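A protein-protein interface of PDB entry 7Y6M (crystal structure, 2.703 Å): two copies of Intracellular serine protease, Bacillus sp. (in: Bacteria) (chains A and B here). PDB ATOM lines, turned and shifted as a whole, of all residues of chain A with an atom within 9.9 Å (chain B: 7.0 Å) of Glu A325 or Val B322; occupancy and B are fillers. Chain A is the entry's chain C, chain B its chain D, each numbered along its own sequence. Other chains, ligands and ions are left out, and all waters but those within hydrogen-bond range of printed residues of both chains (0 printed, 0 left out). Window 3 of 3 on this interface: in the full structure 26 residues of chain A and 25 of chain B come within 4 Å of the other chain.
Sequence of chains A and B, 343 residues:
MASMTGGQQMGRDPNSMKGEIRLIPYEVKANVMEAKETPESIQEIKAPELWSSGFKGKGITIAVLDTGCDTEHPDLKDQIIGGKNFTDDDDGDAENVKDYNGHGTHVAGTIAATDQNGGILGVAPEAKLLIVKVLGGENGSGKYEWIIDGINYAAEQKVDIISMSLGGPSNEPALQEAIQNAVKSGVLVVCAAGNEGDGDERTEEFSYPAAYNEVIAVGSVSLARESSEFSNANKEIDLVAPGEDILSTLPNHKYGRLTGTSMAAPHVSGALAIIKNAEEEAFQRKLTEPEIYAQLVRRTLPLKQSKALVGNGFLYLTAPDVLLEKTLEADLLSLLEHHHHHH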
ATOM      1  N   THR A 300     -25.619   0.852  20.667  1.00  0.00           N
ATOM      2  CA  THR A 300     -27.049   0.824  20.377  1.00  0.00           C
ATOM      3  C   THR A 300     -27.814   0.426  21.633  1.00  0.00           C
ATOM      4  O   THR A 300     -27.591  -0.662  22.182  1.00  0.00           O
ATOM      5  CB  THR A 300     -27.331  -0.156  19.231  1.00  0.00           C
ATOM      6  OG1 THR A 300     -26.777   0.367  18.019  1.00  0.00           O
ATOM      7  CG2 THR A 300     -28.808  -0.371  19.048  1.00  0.00           C
ATOM      8  N   LEU A 301     -28.744   1.339  22.119  1.00  0.00           N
ATOM      9  CA  LEU A 301     -29.472   0.616  23.153  1.00  0.00           C
ATOM     10  C   LEU A 301     -30.742  -0.008  22.577  1.00  0.00           C
ATOM     11  O   LEU A 301     -31.350   0.540  21.652  1.00  0.00           O
ATOM     12  CB  LEU A 301     -29.826   1.543  24.317  1.00  0.00           C
ATOM     13  CG  LEU A 301     -30.487   2.888  24.051  1.00  0.00           C
ATOM     14  CD1 LEU A 301     -31.983   2.763  24.221  1.00  0.00           C
ATOM     15  CD2 LEU A 301     -29.930   3.949  24.999  1.00  0.00           C
ATOM     16  N   PRO A 302     -31.174  -1.160  23.075  1.00  0.00           N
ATOM     17  CA  PRO A 302     -32.368  -1.790  22.511  1.00  0.00           C
ATOM     18  C   PRO A 302     -33.629  -1.055  22.933  1.00  0.00           C
ATOM     19  O   PRO A 302     -33.670  -0.337  23.935  1.00  0.00           O
ATOM     20  CB  PRO A 302     -32.334  -3.203  23.101  1.00  0.00           C
ATOM     21  CG  PRO A 302     -31.668  -3.022  24.428  1.00  0.00           C
ATOM     22  CD  PRO A 302     -30.676  -1.887  24.258  1.00  0.00           C
ATOM     23  N   THR A 318     -22.736   6.212  23.477  1.00  0.00           N
ATOM     24  CA  THR A 318     -22.125   6.020  24.793  1.00  0.00           C
ATOM     25  C   THR A 318     -22.654   4.775  25.502  1.00  0.00           C
ATOM     26  O   THR A 318     -22.486   4.627  26.718  1.00  0.00           O
ATOM     27  CB  THR A 318     -22.317   7.258  25.679  1.00  0.00           C
ATOM     28  OG1 THR A 318     -23.677   7.707  25.629  1.00  0.00           O
ATOM     29  CG2 THR A 318     -21.408   8.383  25.224  1.00  0.00           C
ATOM     30  N   ALA A 319     -23.269   3.866  24.754  1.00  0.00           N
ATOM     31  CA  ALA A 319     -23.838   2.668  25.358  1.00  0.00           C
ATOM     32  C   ALA A 319     -22.838   1.817  26.148  1.00  0.00           C
ATOM     33  O   ALA A 319     -23.213   1.324  27.227  1.00  0.00           O
ATOM     34  CB  ALA A 319     -24.526   1.853  24.255  1.00  0.00           C
ATOM     35  N   PRO A 320     -21.598   1.586  25.702  1.00  0.00           N
ATOM     36  CA  PRO A 320     -20.722   0.732  26.520  1.00  0.00           C
ATOM     37  C   PRO A 320     -20.361   1.375  27.843  1.00  0.00           C
ATOM     38  O   PRO A 320     -20.305   0.692  28.874  1.00  0.00           O
ATOM     39  CB  PRO A 320     -19.495   0.529  25.623  1.00  0.00           C
ATOM     40  CG  PRO A 320     -19.473   1.751  24.769  1.00  0.00           C
ATOM     41  CD  PRO A 320     -20.905   2.056  24.485  1.00  0.00           C
ATOM     42  N   ASP A 321     -20.110   2.682  27.849  1.00  0.00           N
ATOM     43  CA  ASP A 321     -19.842   3.360  29.110  1.00  0.00           C
ATOM     44  C   ASP A 321     -20.981   3.125  30.090  1.00  0.00           C
ATOM     45  O   ASP A 321     -20.766   2.625  31.201  1.00  0.00           O
ATOM     46  CB  ASP A 321     -19.604   4.840  28.841  1.00  0.00           C
ATOM     47  CG  ASP A 321     -18.536   5.043  27.791  1.00  0.00           C
ATOM     48  OD1 ASP A 321     -17.380   4.696  28.107  1.00  0.00           O
ATOM     49  OD2 ASP A 321     -18.848   5.490  26.653  1.00  0.00           O
ATOM     50  N   VAL A 322     -22.211   3.403  29.659  1.00  0.00           N
ATOM     51  CA  VAL A 322     -23.432   3.077  30.391  1.00  0.00           C
ATOM     52  C   VAL A 322     -23.372   1.680  31.001  1.00  0.00           C
ATOM     53  O   VAL A 322     -23.957   1.434  32.064  1.00  0.00           O
ATOM     54  CB  VAL A 322     -24.648   3.211  29.460  1.00  0.00           C
ATOM     55  CG1 VAL A 322     -25.927   2.853  30.187  1.00  0.00           C
ATOM     56  CG2 VAL A 322     -24.691   4.625  28.881  1.00  0.00           C
ATOM     57  N   LEU A 323     -22.660   0.759  30.336  1.00  0.00           N
ATOM     58  CA  LEU A 323     -22.478  -0.585  30.881  1.00  0.00           C
ATOM     59  C   LEU A 323     -21.471  -0.585  32.024  1.00  0.00           C
ATOM     60  O   LEU A 323     -21.614  -1.353  32.986  1.00  0.00           O
ATOM     61  CB  LEU A 323     -22.026  -1.546  29.781  1.00  0.00           C
ATOM     62  CG  LEU A 323     -22.647  -2.934  29.739  1.00  0.00           C
ATOM     63  CD1 LEU A 323     -24.107  -2.780  29.351  1.00  0.00           C
ATOM     64  CD2 LEU A 323     -21.903  -3.855  28.773  1.00  0.00           C
ATOM     65  N   LEU A 324     -20.438   0.260  31.936  1.00  0.00           N
ATOM     66  CA  LEU A 324     -19.481   0.350  33.039  1.00  0.00           C
ATOM     67  C   LEU A 324     -20.110   1.010  34.266  1.00  0.00           C
ATOM     68  O   LEU A 324     -19.841   0.599  35.404  1.00  0.00           O
ATOM     69  CB  LEU A 324     -18.228   1.111  32.598  1.00  0.00           C
ATOM     70  CG  LEU A 324     -17.371   0.428  31.523  1.00  0.00           C
ATOM     71  CD1 LEU A 324     -15.891   0.819  31.630  1.00  0.00           C
ATOM     72  CD2 LEU A 324     -17.543  -1.090  31.572  1.00  0.00           C
ATOM     73  N   GLU A 325     -20.963   2.019  34.044  1.00  0.00           N
ATOM     74  CA  GLU A 325     -21.647   2.792  35.095  1.00  0.00           C
ATOM     75  C   GLU A 325     -20.649   3.526  36.003  1.00  0.00           C
ATOM     76  O   GLU A 325     -20.757   4.738  36.242  1.00  0.00           O
ATOM     77  CB  GLU A 325     -22.563   1.888  35.939  1.00  0.00           C
ATOM     78  CG  GLU A 325     -23.537   1.021  35.139  1.00  0.00           C
ATOM     79  CD  GLU A 325     -23.878  -0.287  35.848  1.00  0.00           C
ATOM     80  OE1 GLU A 325     -24.529  -1.154  35.219  1.00  0.00           O
ATOM     81  OE2 GLU A 325     -23.494  -0.445  37.031  1.00  0.00           O
ATOM     82  N   LYS B  46     -23.077 -15.719  32.671  1.00  0.00           N
ATOM     83  CA  LYS B  46     -24.501 -15.428  32.651  1.00  0.00           C
ATOM     84  C   LYS B  46     -25.289 -16.383  31.766  1.00  0.00           C
ATOM     85  O   LYS B  46     -26.421 -16.067  31.361  1.00  0.00           O
ATOM     86  CB  LYS B  46     -24.774 -13.977  32.235  1.00  0.00           C
ATOM     87  CG  LYS B  46     -24.566 -12.972  33.360  1.00  0.00           C
ATOM     88  CD  LYS B  46     -25.065 -13.536  34.681  1.00  0.00           C
ATOM     89  CE  LYS B  46     -25.121 -12.472  35.752  1.00  0.00           C
ATOM     90  NZ  LYS B  46     -23.901 -11.623  35.701  1.00  0.00           N
ATOM     91  N   LEU B 301     -18.690  -7.069  27.876  1.00  0.00           N
ATOM     92  CA  LEU B 301     -18.658  -6.038  28.950  1.00  0.00           C
ATOM     93  C   LEU B 301     -17.329  -5.275  28.883  1.00  0.00           C
ATOM     94  O   LEU B 301     -16.272  -5.916  29.047  1.00  0.00           O
ATOM     95  CB  LEU B 301     -18.829  -6.728  30.307  1.00  0.00           C
ATOM     96  CG  LEU B 301     -18.919  -5.792  31.512  1.00  0.00           C
ATOM     97  CD1 LEU B 301     -20.345  -5.716  32.034  1.00  0.00           C
ATOM     98  CD2 LEU B 301     -17.970  -6.237  32.615  1.00  0.00           C
ATOM     99  N   TYR B 316     -20.206 -11.816  28.590  1.00  0.00           N
ATOM    100  CA  TYR B 316     -21.174 -11.474  29.631  1.00  0.00           C
ATOM    101  C   TYR B 316     -22.550 -11.365  28.966  1.00  0.00           C
ATOM    102  O   TYR B 316     -22.920 -10.312  28.440  1.00  0.00           O
ATOM    103  CB  TYR B 316     -20.736 -10.182  30.325  1.00  0.00           C
ATOM    104  CG  TYR B 316     -21.458  -9.818  31.617  1.00  0.00           C
ATOM    105  CD1 TYR B 316     -21.011 -10.289  32.851  1.00  0.00           C
ATOM    106  CD2 TYR B 316     -22.564  -8.958  31.604  1.00  0.00           C
ATOM    107  CE1 TYR B 316     -21.655  -9.934  34.031  1.00  0.00           C
ATOM    108  CE2 TYR B 316     -23.214  -8.602  32.775  1.00  0.00           C
ATOM    109  CZ  TYR B 316     -22.752  -9.092  33.983  1.00  0.00           C
ATOM    110  OH  TYR B 316     -23.390  -8.740  35.146  1.00  0.00           O
ATOM    111  N   THR B 318     -25.813 -11.323  29.500  1.00  0.00           N
ATOM    112  CA  THR B 318     -26.941 -10.437  29.783  1.00  0.00           C
ATOM    113  C   THR B 318     -26.607  -8.968  29.547  1.00  0.00           C
ATOM    114  O   THR B 318     -27.431  -8.109  29.865  1.00  0.00           O
ATOM    115  CB  THR B 318     -27.441 -10.620  31.226  1.00  0.00           C
ATOM    116  OG1 THR B 318     -26.381 -10.372  32.161  1.00  0.00           O
ATOM    117  CG2 THR B 318     -27.978 -12.028  31.435  1.00  0.00           C
ATOM    118  N   ALA B 319     -25.440  -8.672  28.974  1.00  0.00           N
ATOM    119  CA  ALA B 319     -24.938  -7.299  28.961  1.00  0.00           C
ATOM    120  C   ALA B 319     -25.882  -6.271  28.335  1.00  0.00           C
ATOM    121  O   ALA B 319     -25.937  -5.146  28.858  1.00  0.00           O
ATOM    122  CB  ALA B 319     -23.565  -7.255  28.273  1.00  0.00           C
ATOM    123  N   PRO B 320     -26.616  -6.544  27.250  1.00  0.00           N
ATOM    124  CA  PRO B 320     -27.546  -5.527  26.745  1.00  0.00           C
ATOM    125  C   PRO B 320     -28.852  -5.453  27.521  1.00  0.00           C
ATOM    126  O   PRO B 320     -29.621  -4.507  27.304  1.00  0.00           O
ATOM    127  CB  PRO B 320     -27.775  -5.953  25.286  1.00  0.00           C
ATOM    128  CG  PRO B 320     -27.600  -7.387  25.297  1.00  0.00           C
ATOM    129  CD  PRO B 320     -26.540  -7.689  26.326  1.00  0.00           C
ATOM    130  N   ASP B 321     -29.124  -6.412  28.413  1.00  0.00           N
ATOM    131  CA  ASP B 321     -30.204  -6.238  29.380  1.00  0.00           C
ATOM    132  C   ASP B 321     -29.813  -5.225  30.447  1.00  0.00           C
ATOM    133  O   ASP B 321     -30.635  -4.403  30.860  1.00  0.00           O
ATOM    134  CB  ASP B 321     -30.578  -7.582  30.014  1.00  0.00           C
ATOM    135  CG  ASP B 321     -31.343  -8.490  29.056  1.00  0.00           C
ATOM    136  OD1 ASP B 321     -32.584  -8.330  28.944  1.00  0.00           O
ATOM    137  OD2 ASP B 321     -30.704  -9.357  28.411  1.00  0.00           O
ATOM    138  N   VAL B 322     -28.555  -5.254  30.887  1.00  0.00           N
ATOM    139  CA  VAL B 322     -27.971  -4.255  31.786  1.00  0.00           C
ATOM    140  C   VAL B 322     -28.109  -2.843  31.217  1.00  0.00           C
ATOM    141  O   VAL B 322     -27.922  -1.850  31.933  1.00  0.00           O
ATOM    142  CB  VAL B 322     -26.494  -4.585  32.050  1.00  0.00           C
ATOM    143  CG1 VAL B 322     -25.965  -3.822  33.253  1.00  0.00           C
ATOM    144  CG2 VAL B 322     -26.327  -6.082  32.226  1.00  0.00           C
ATOM    145  N   LEU B 323     -28.420  -2.743  29.923  1.00  0.00           N
ATOM    146  CA  LEU B 323     -28.605  -1.473  29.235  1.00  0.00           C
ATOM    147  C   LEU B 323     -30.046  -0.982  29.355  1.00  0.00           C
ATOM    148  O   LEU B 323     -30.286   0.221  29.524  1.00  0.00           O
ATOM    149  CB  LEU B 323     -28.201  -1.626  27.765  1.00  0.00           C
ATOM    150  CG  LEU B 323     -27.332  -0.571  27.072  1.00  0.00           C
ATOM    151  CD1 LEU B 323     -26.278   0.039  27.995  1.00  0.00           C
ATOM    152  CD2 LEU B 323     -26.682  -1.206  25.867  1.00  0.00           C
ATOM    153  N   LEU B 324     -31.014  -1.896  29.274  1.00  0.00           N
ATOM    154  CA  LEU B 324     -32.347  -1.623  29.794  1.00  0.00           C
ATOM    155  C   LEU B 324     -32.254  -1.284  31.281  1.00  0.00           C
ATOM    156  O   LEU B 324     -32.165  -2.185  32.128  1.00  0.00           O
ATOM    157  CB  LEU B 324     -33.273  -2.824  29.577  1.00  0.00           C
ATOM    158  CG  LEU B 324     -33.138  -3.568  28.249  1.00  0.00           C
ATOM    159  CD1 LEU B 324     -33.655  -5.003  28.365  1.00  0.00           C
ATOM    160  CD2 LEU B 324     -33.864  -2.825  27.137  1.00  0.00           C
ATOM    161  N   GLU B 325     -32.253   0.009  31.607  1.00  0.00           N
ATOM    162  CA  GLU B 325     -32.236   0.441  33.003  1.00  0.00           C
ATOM    163  C   GLU B 325     -32.795   1.868  33.170  1.00  0.00           C
ATOM    164  O   GLU B 325     -32.054   2.841  33.343  1.00  0.00           O
ATOM    165  CB  GLU B 325     -30.815   0.344  33.556  1.00  0.00           C
ATOM    166  CG  GLU B 325     -30.735   0.187  35.061  1.00  0.00           C
ATOM    167  CD  GLU B 325     -29.516   0.876  35.626  1.00  0.00           C
ATOM    168  OE1 GLU B 325     -28.568   1.106  34.842  1.00  0.00           O
ATOM    169  OE2 GLU B 325     -29.511   1.203  36.833  1.00  0.00           O
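Hydrophobic or aromatic side chains of chain B within 4 Å of the printed part of chain A: Ala B319, Val B322, Leu B323 and Leu B324. Along chain B the printed residues that touch a printed residue of chain A span positions 301 to 324. Printed residues of chain A that touch a printed residue of chain B: Thr A300, Pro A302, Ala A319, Val A322, Leu A323 and Glu A325. Hydrophobic or aromatic side chains of chain A within 4 Å of the printed part of chain B: Pro A302, Val A322 and Leu A323. Among the printed residues, no Asp or Glu carboxylate lies within 4 Å of a Lys or Arg side-chain nitrogen of the other chain.
Ala A319 touches Leu B323, and with the chains exchanged Leu A323 touches Ala B319. Val A322 touches Leu B323, but with the chains exchanged Leu A323 does not touch Val B322 (4.03 Å). Leu A323 touches Leu B301, but with the chains exchanged Leu A301 does not touch Leu B323 (4.3 Å). Glu A325 touches Val B322, but with the chains exchanged Val A322 does not touch Glu B325 (5.4 Å).
Glu A325 touches one residue of chain B. Val B322 touches one residue of chain A. Of chain A, only Leu A323 (3.0 Å) comes within 4 Å of Ala B319. Leu B323 touches just these residues of chain A: Thr A300, Ala A319, Val A322 and Leu A323. Printed residues of chain A within 4 Å of Leu B324: Pro A302 (3.5 Å). Printed residues of chain B within 4 Å of Pro A302: Pro B320 and Leu B324. Of the printed residues of chain B, Ala A319 touches Leu B323 (3.4 Å). Thr B318 touches none of the printed residues of chain A. The nearest printed residue of chain B that does not touch Val A322 is Val B322 (5.2 Å).
Among the printed residues, merely in contact across the chains: Leu A323 with Ala B319, Ala A319 with Leu B323, Pro A302 with Leu B324, Val A322 with Leu B323, Glu A325 with Val B322, Leu A323 with Leu B323, Pro A302 with Pro B320, Thr A300 with Leu B323 and Leu A323 with Leu B301.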
